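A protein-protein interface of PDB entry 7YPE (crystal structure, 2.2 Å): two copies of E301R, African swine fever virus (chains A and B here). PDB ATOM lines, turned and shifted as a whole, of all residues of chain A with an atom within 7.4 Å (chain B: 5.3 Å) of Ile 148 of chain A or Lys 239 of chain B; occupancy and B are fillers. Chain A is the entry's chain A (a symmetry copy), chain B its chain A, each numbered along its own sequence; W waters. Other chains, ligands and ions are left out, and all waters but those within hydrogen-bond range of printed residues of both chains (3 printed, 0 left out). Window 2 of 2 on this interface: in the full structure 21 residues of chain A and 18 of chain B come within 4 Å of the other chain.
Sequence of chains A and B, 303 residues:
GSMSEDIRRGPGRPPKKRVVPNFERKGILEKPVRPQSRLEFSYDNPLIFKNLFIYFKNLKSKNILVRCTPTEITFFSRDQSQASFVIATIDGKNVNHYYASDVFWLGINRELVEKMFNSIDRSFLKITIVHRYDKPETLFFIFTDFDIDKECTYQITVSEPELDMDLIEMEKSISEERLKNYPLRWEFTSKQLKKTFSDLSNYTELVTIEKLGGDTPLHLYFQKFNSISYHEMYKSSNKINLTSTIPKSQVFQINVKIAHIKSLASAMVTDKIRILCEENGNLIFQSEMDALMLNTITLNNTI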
ATOM      1  N   SER A   2       1.381  -9.639  14.059  1.00  0.00           N
ATOM      2  CA  SER A   2       0.025  -9.549  14.566  1.00  0.00           C
ATOM      3  C   SER A   2      -0.993 -10.220  13.667  1.00  0.00           C
ATOM      4  O   SER A   2      -0.962 -11.435  13.477  1.00  0.00           O
ATOM      5  N   MET A   3      -1.901  -9.423  13.112  1.00  0.00           N
ATOM      6  CA  MET A   3      -2.924  -9.933  12.207  1.00  0.00           C
ATOM      7  C   MET A   3      -2.744  -9.329  10.816  1.00  0.00           C
ATOM      8  O   MET A   3      -3.064  -8.162  10.593  1.00  0.00           O
ATOM      9  CB  MET A   3      -4.321  -9.629  12.751  1.00  0.00           C
ATOM     10  CG  MET A   3      -5.434 -10.387  12.055  1.00  0.00           C
ATOM     11  SD  MET A   3      -6.043 -11.943  13.064  1.00  0.00           S
ATOM     12  CE  MET A   3      -7.715 -11.227  13.772  1.00  0.00           C
ATOM     13  N   SER A   4      -2.228 -10.129   9.884  1.00  0.00           N
ATOM     14  CA  SER A   4      -1.850  -9.648   8.564  1.00  0.00           C
ATOM     15  C   SER A   4      -2.543 -10.461   7.478  1.00  0.00           C
ATOM     16  O   SER A   4      -2.793 -11.658   7.638  1.00  0.00           O
ATOM     17  CB  SER A   4      -0.330  -9.714   8.364  1.00  0.00           C
ATOM     18  OG  SER A   4      -0.005  -9.994   7.012  1.00  0.00           O
ATOM     19  N   VAL A  19      -0.530  -5.566   7.072  1.00  0.00           N
ATOM     20  CA  VAL A  19      -1.071  -5.834   8.400  1.00  0.00           C
ATOM     21  C   VAL A  19      -2.459  -5.218   8.498  1.00  0.00           C
ATOM     22  O   VAL A  19      -2.644  -4.031   8.205  1.00  0.00           O
ATOM     23  CB  VAL A  19      -0.142  -5.284   9.494  1.00  0.00           C
ATOM     24  CG1 VAL A  19      -0.892  -5.140  10.812  1.00  0.00           C
ATOM     25  CG2 VAL A  19       1.066  -6.188   9.662  1.00  0.00           C
ATOM     26  N   SER A 123       3.990   3.399   5.748  1.00  0.00           N
ATOM     27  CA  SER A 123       4.490   2.263   6.515  1.00  0.00           C
ATOM     28  C   SER A 123       4.220   2.416   8.007  1.00  0.00           C
ATOM     29  O   SER A 123       4.316   1.431   8.745  1.00  0.00           O
ATOM     30  CB  SER A 123       5.990   2.076   6.272  1.00  0.00           C
ATOM     31  OG  SER A 123       6.752   3.076   6.927  1.00  0.00           O
ATOM     32  N   ASP A 145       5.738   0.671  12.786  1.00  0.00           N
ATOM     33  CA  ASP A 145       5.557  -0.097  11.560  1.00  0.00           C
ATOM     34  C   ASP A 145       5.122  -1.501  11.966  1.00  0.00           C
ATOM     35  O   ASP A 145       5.929  -2.285  12.474  1.00  0.00           O
ATOM     36  CB  ASP A 145       6.852  -0.124  10.746  1.00  0.00           C
ATOM     37  CG  ASP A 145       6.711  -0.864   9.417  1.00  0.00           C
ATOM     38  OD1 ASP A 145       5.774  -1.675   9.254  1.00  0.00           O
ATOM     39  OD2 ASP A 145       7.558  -0.635   8.529  1.00  0.00           O
ATOM     40  N   PHE A 146       3.847  -1.817  11.734  1.00  0.00           N
ATOM     41  CA  PHE A 146       3.293  -3.095  12.165  1.00  0.00           C
ATOM     42  C   PHE A 146       3.657  -4.252  11.243  1.00  0.00           C
ATOM     43  O   PHE A 146       3.491  -5.409  11.642  1.00  0.00           O
ATOM     44  CB  PHE A 146       1.771  -2.986  12.285  1.00  0.00           C
ATOM     45  CG  PHE A 146       1.316  -2.194  13.477  1.00  0.00           C
ATOM     46  CD1 PHE A 146       1.196  -2.795  14.721  1.00  0.00           C
ATOM     47  CD2 PHE A 146       1.014  -0.848  13.358  1.00  0.00           C
ATOM     48  CE1 PHE A 146       0.781  -2.068  15.820  1.00  0.00           C
ATOM     49  CE2 PHE A 146       0.597  -0.115  14.455  1.00  0.00           C
ATOM     50  CZ  PHE A 146       0.481  -0.727  15.688  1.00  0.00           C
ATOM     51  N   ASP A 147       4.146  -3.975  10.031  1.00  0.00           N
ATOM     52  CA  ASP A 147       4.555  -5.053   9.136  1.00  0.00           C
ATOM     53  C   ASP A 147       5.724  -5.836   9.718  1.00  0.00           C
ATOM     54  O   ASP A 147       5.781  -7.066   9.595  1.00  0.00           O
ATOM     55  CB  ASP A 147       4.921  -4.490   7.764  1.00  0.00           C
ATOM     56  CG  ASP A 147       3.729  -3.906   7.036  1.00  0.00           C
ATOM     57  OD1 ASP A 147       2.604  -4.409   7.240  1.00  0.00           O
ATOM     58  OD2 ASP A 147       3.916  -2.944   6.263  1.00  0.00           O
ATOM     59  N   ILE A 148       6.665  -5.144  10.360  1.00  0.00           N
ATOM     60  CA  ILE A 148       7.852  -5.766  10.924  1.00  0.00           C
ATOM     61  C   ILE A 148       7.999  -5.476  12.414  1.00  0.00           C
ATOM     62  O   ILE A 148       9.046  -5.759  12.994  1.00  0.00           O
ATOM     63  CB  ILE A 148       9.120  -5.336  10.160  1.00  0.00           C
ATOM     64  CG1 ILE A 148       9.131  -3.818   9.966  1.00  0.00           C
ATOM     65  CG2 ILE A 148       9.198  -6.046   8.817  1.00  0.00           C
ATOM     66  CD1 ILE A 148      10.334  -3.308   9.204  1.00  0.00           C
ATOM     67  N   ASP A 149       6.961  -4.925  13.045  1.00  0.00           N
ATOM     68  CA  ASP A 149       6.998  -4.526  14.455  1.00  0.00           C
ATOM     69  C   ASP A 149       8.211  -3.646  14.746  1.00  0.00           C
ATOM     70  O   ASP A 149       8.951  -3.855  15.710  1.00  0.00           O
ATOM     71  CB  ASP A 149       6.972  -5.743  15.384  1.00  0.00           C
ATOM     72  CG  ASP A 149       5.656  -6.491  15.327  1.00  0.00           C
ATOM     73  OD1 ASP A 149       4.608  -5.873  15.609  1.00  0.00           O
ATOM     74  OD2 ASP A 149       5.665  -7.690  14.986  1.00  0.00           O
ATOM     75  N   LYS A 150       8.415  -2.649  13.892  1.00  0.00           N
ATOM     76  CA  LYS A 150       9.508  -1.699  14.039  1.00  0.00           C
ATOM     77  C   LYS A 150       8.977  -0.440  14.712  1.00  0.00           C
ATOM     78  O   LYS A 150       8.024   0.178  14.222  1.00  0.00           O
ATOM     79  CB  LYS A 150      10.132  -1.366  12.684  1.00  0.00           C
ATOM     80  CG  LYS A 150      10.896  -0.052  12.665  1.00  0.00           C
ATOM     81  CD  LYS A 150      11.572   0.172  11.325  1.00  0.00           C
ATOM     82  CE  LYS A 150      10.740   1.074  10.432  1.00  0.00           C
ATOM     83  NZ  LYS A 150      11.404   1.323   9.123  1.00  0.00           N
ATOM     84  N   GLU A 151       9.590  -0.067  15.832  1.00  0.00           N
ATOM     85  CA  GLU A 151       9.203   1.107  16.603  1.00  0.00           C
ATOM     86  C   GLU A 151      10.280   2.172  16.448  1.00  0.00           C
ATOM     87  O   GLU A 151      11.436   1.946  16.823  1.00  0.00           O
ATOM     88  CB  GLU A 151       9.010   0.750  18.076  1.00  0.00           C
ATOM     89  CG  GLU A 151       7.682   1.185  18.659  1.00  0.00           C
ATOM     90  CD  GLU A 151       7.454   0.628  20.049  1.00  0.00           C
ATOM     91  OE1 GLU A 151       8.234   0.973  20.960  1.00  0.00           O
ATOM     92  OE2 GLU A 151       6.497  -0.154  20.229  1.00  0.00           O
ATOM     93  N   PHE B 188      16.322  -7.080   5.166  1.00  0.00           N
ATOM     94  CA  PHE B 188      15.436  -5.963   4.882  1.00  0.00           C
ATOM     95  C   PHE B 188      14.963  -6.045   3.440  1.00  0.00           C
ATOM     96  O   PHE B 188      15.702  -6.486   2.555  1.00  0.00           O
ATOM     97  CB  PHE B 188      16.138  -4.614   5.087  1.00  0.00           C
ATOM     98  CG  PHE B 188      16.094  -4.106   6.495  1.00  0.00           C
ATOM     99  CD1 PHE B 188      15.230  -4.658   7.424  1.00  0.00           C
ATOM    100  CD2 PHE B 188      16.916  -3.062   6.886  1.00  0.00           C
ATOM    101  CE1 PHE B 188      15.194  -4.185   8.720  1.00  0.00           C
ATOM    102  CE2 PHE B 188      16.882  -2.584   8.177  1.00  0.00           C
ATOM    103  CZ  PHE B 188      16.022  -3.147   9.095  1.00  0.00           C
ATOM    104  N   GLN B 192      12.552  -1.097   3.000  1.00  0.00           N
ATOM    105  CA  GLN B 192      12.844  -0.908   4.418  1.00  0.00           C
ATOM    106  C   GLN B 192      14.253  -0.369   4.628  1.00  0.00           C
ATOM    107  O   GLN B 192      14.458   0.540   5.440  1.00  0.00           O
ATOM    108  CB  GLN B 192      12.655  -2.225   5.170  1.00  0.00           C
ATOM    109  CG  GLN B 192      11.201  -2.605   5.385  1.00  0.00           C
ATOM    110  CD  GLN B 192      11.005  -4.101   5.506  1.00  0.00           C
ATOM    111  OE1 GLN B 192      11.944  -4.878   5.325  1.00  0.00           O
ATOM    112  NE2 GLN B 192       9.780  -4.516   5.809  1.00  0.00           N
ATOM    113  N   TYR B 234      13.464  -3.150  16.578  1.00  0.00           N
ATOM    114  CA  TYR B 234      12.780  -4.237  15.883  1.00  0.00           C
ATOM    115  C   TYR B 234      12.373  -5.272  16.927  1.00  0.00           C
ATOM    116  O   TYR B 234      13.179  -6.109  17.340  1.00  0.00           O
ATOM    117  CB  TYR B 234      13.677  -4.813  14.792  1.00  0.00           C
ATOM    118  CG  TYR B 234      13.931  -3.809  13.689  1.00  0.00           C
ATOM    119  CD1 TYR B 234      14.916  -2.838  13.819  1.00  0.00           C
ATOM    120  CD2 TYR B 234      13.160  -3.807  12.533  1.00  0.00           C
ATOM    121  CE1 TYR B 234      15.141  -1.906  12.824  1.00  0.00           C
ATOM    122  CE2 TYR B 234      13.379  -2.880  11.531  1.00  0.00           C
ATOM    123  CZ  TYR B 234      14.369  -1.932  11.683  1.00  0.00           C
ATOM    124  OH  TYR B 234      14.588  -1.005  10.688  1.00  0.00           O
ATOM    125  N   LYS B 235      11.109  -5.204  17.350  1.00  0.00           N
ATOM    126  CA  LYS B 235      10.616  -5.988  18.475  1.00  0.00           C
ATOM    127  C   LYS B 235      10.281  -7.428  18.112  1.00  0.00           C
ATOM    128  O   LYS B 235       9.956  -8.212  19.009  1.00  0.00           O
ATOM    129  CB  LYS B 235       9.378  -5.310  19.071  1.00  0.00           C
ATOM    130  CG  LYS B 235       9.645  -3.923  19.636  1.00  0.00           C
ATOM    131  CD  LYS B 235       8.416  -3.356  20.329  1.00  0.00           C
ATOM    132  CE  LYS B 235       7.225  -3.298  19.384  1.00  0.00           C
ATOM    133  NZ  LYS B 235       6.039  -2.661  20.021  1.00  0.00           N
ATOM    134  N   SER B 236      10.350  -7.797  16.835  1.00  0.00           N
ATOM    135  CA  SER B 236      10.077  -9.164  16.393  1.00  0.00           C
ATOM    136  C   SER B 236      11.190  -9.576  15.435  1.00  0.00           C
ATOM    137  O   SER B 236      11.150  -9.242  14.247  1.00  0.00           O
ATOM    138  CB  SER B 236       8.704  -9.268  15.736  1.00  0.00           C
ATOM    139  OG  SER B 236       7.675  -9.030  16.681  1.00  0.00           O
ATOM    140  N   SER B 237      12.181 -10.302  15.958  1.00  0.00           N
ATOM    141  CA  SER B 237      13.329 -10.689  15.144  1.00  0.00           C
ATOM    142  C   SER B 237      12.933 -11.626  14.011  1.00  0.00           C
ATOM    143  O   SER B 237      13.578 -11.630  12.956  1.00  0.00           O
ATOM    144  CB  SER B 237      14.397 -11.338  16.025  1.00  0.00           C
ATOM    145  OG  SER B 237      14.873 -10.423  16.996  1.00  0.00           O
ATOM    146  N   ASN B 238      11.882 -12.427  14.206  1.00  0.00           N
ATOM    147  CA  ASN B 238      11.440 -13.333  13.152  1.00  0.00           C
ATOM    148  C   ASN B 238      10.941 -12.576  11.928  1.00  0.00           C
ATOM    149  O   ASN B 238      11.052 -13.074  10.801  1.00  0.00           O
ATOM    150  CB  ASN B 238      10.344 -14.257  13.682  1.00  0.00           C
ATOM    151  CG  ASN B 238       9.179 -13.492  14.283  1.00  0.00           C
ATOM    152  OD1 ASN B 238       9.369 -12.599  15.108  1.00  0.00           O
ATOM    153  ND2 ASN B 238       7.966 -13.839  13.869  1.00  0.00           N
ATOM    154  N   LYS B 239      10.393 -11.376  12.121  1.00  0.00           N
ATOM    155  CA  LYS B 239       9.814 -10.625  11.015  1.00  0.00           C
ATOM    156  C   LYS B 239      10.859  -9.951  10.137  1.00  0.00           C
ATOM    157  O   LYS B 239      10.514  -9.478   9.048  1.00  0.00           O
ATOM    158  CB  LYS B 239       8.827  -9.587  11.552  1.00  0.00           C
ATOM    159  CG  LYS B 239       7.541 -10.213  12.061  1.00  0.00           C
ATOM    160  CD  LYS B 239       6.464  -9.180  12.321  1.00  0.00           C
ATOM    161  CE  LYS B 239       5.169  -9.851  12.755  1.00  0.00           C
ATOM    162  NZ  LYS B 239       4.170  -8.863  13.242  1.00  0.00           N
ATOM    163  N   ILE B 240      12.115  -9.897  10.572  1.00  0.00           N
ATOM    164  CA  ILE B 240      13.210  -9.427   9.737  1.00  0.00           C
ATOM    165  C   ILE B 240      14.255 -10.525   9.534  1.00  0.00           C
ATOM    166  O   ILE B 240      15.377 -10.247   9.121  1.00  0.00           O
ATOM    167  CB  ILE B 240      13.844  -8.146  10.313  1.00  0.00           C
ATOM    168  CG1 ILE B 240      14.222  -8.345  11.783  1.00  0.00           C
ATOM    169  CG2 ILE B 240      12.892  -6.968  10.157  1.00  0.00           C
ATOM    170  CD1 ILE B 240      15.184  -7.296  12.312  1.00  0.00           C
ATOM    171  N   ASN B 241      13.885 -11.774   9.825  1.00  0.00           N
ATOM    172  CA  ASN B 241      14.758 -12.934   9.632  1.00  0.00           C
ATOM    173  C   ASN B 241      16.105 -12.737  10.322  1.00  0.00           C
ATOM    174  O   ASN B 241      17.165 -13.014   9.757  1.00  0.00           O
ATOM    175  CB  ASN B 241      14.945 -13.236   8.145  1.00  0.00           C
ATOM    176  CG  ASN B 241      13.745 -13.931   7.537  1.00  0.00           C
ATOM    177  OD1 ASN B 241      13.062 -14.710   8.204  1.00  0.00           O
ATOM    178  ND2 ASN B 241      13.480 -13.654   6.266  1.00  0.00           N
HETATM  179  O   HOH W   1      13.150  -0.489   8.258  1.00  0.00           O
HETATM  180  O   HOH W   2      11.083  -6.673  14.307  1.00  0.00           O
HETATM  181  O   HOH W   3       7.660  -2.292   6.106  1.00  0.00           O
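N of Val 19 of chain A lies within hydrogen-bond range of OD1 of Asp 147 of chain A.
OD1 of Asp 145 of chain A sits at hydrogen-bond distance from N of Asp 147 of chain A, at 2.9 Å.
The backbone carbonyl oxygen (O) of Lys 150 of chain A is in hydrogen-bond range of the backbone NH (N) of Asp 145 of chain A (2.7 Å).
Hydrophobic or aromatic side chains of chain A that line the printed part of chain B: Ile 148.
Along chain A the printed residues that touch a printed residue of chain B span positions 2 to 151.
Among the printed residues, 12 pairs touch across the chains.
Among the printed residues, Asp or Glu carboxylates within 4 Å of a Lys or Arg side-chain nitrogen of the other chain: Asp 149 of chain A with Lys 239 of chain B and Glu 151 of chain A with Lys 235 of chain B.
N of Lys 235 of chain B sits at hydrogen-bond distance from O of Asp 149 of chain A, at 3.0 Å.
The side-chain carboxylate of Glu 151 of chain A lies within salt-bridge range of the side-chain amino group of Lys 235 of chain B, at 2.6 Å.
The side-chain hydroxyl of Ser 236 of chain B lies within hydrogen-bond range of the side-chain carboxylate of Asp 149 of chain A (3.0 Å).
The side-chain carboxylate (OD2) of Asp 149 of chain A is in salt-bridge range of the side-chain amino group (NZ) of Lys 239 of chain B (2.6 Å).
N of Ser 2 of chain A sits close to NZ of Lys 239 of chain B (3.0 Å).
No position is printed for both chains.
Of the 12 pairs that touch across the chains among the printed residues, none has its exchanged pair printed and touching as well.
Among the printed residues, pairs that only touch across the chains: Phe 146 of chain A with Lys 239 of chain B, Asp 147 of chain A with Lys 239 of chain B, Ile 148 of chain A with Gln 192 of chain B, Ile 148 of chain A with Tyr 234 of chain B, Ile 148 of chain A with Lys 239 of chain B, Asp 149 of chain A with Tyr 234 of chain B and Lys 150 of chain A with Tyr 234 of chain B.
Of the printed residues of chain B, Ser 2 of chain A touches Lys 239.
Ser 4 of chain A touches none of the printed residues of chain B.
Of chain B, only Gln 192, Tyr 234 and Lys 239 come within 4 Å of Ile 148 of chain A.
Of the printed residues of chain B, Lys 150 of chain A touches Tyr 234 (3.3 Å).
Of the printed residues of chain A, Gln 192 of chain B touches Ile 148 (3.4 Å).
Of the printed residues of chain A, Tyr 234 of chain B touches Ile 148 (3.9 Å), Asp 149 (3.9 Å) and Lys 150 (3.3 Å).
Printed residues of chain A within 4 Å of Lys 235 of chain B: Asp 149 and Glu 151.
Of chain A, only Ser 2, Phe 146, Asp 147, Ile 148 and Asp 149 come within 4 Å of Lys 239 of chain B.
Water W2 lies within hydrogen-bond range of O of Ser 236 of chain B (2.6 Å), O of Ile 148 of chain A (2.6 Å) and N of Lys 235 of chain B (3.4 Å).
Water W1 lies within hydrogen-bond range of NZ of Lys 150 of chain A (2.7 Å), OH of Tyr 234 of chain B (2.9 Å) and O of Gln 192 of chain B (3.3 Å).
Water W3 bridges the side-chain carboxylate (OD2) of Asp 145 of chain A (2.9 Å) and the side-chain amide nitrogen (NE2) of Gln 192 of chain B (3.1 Å).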
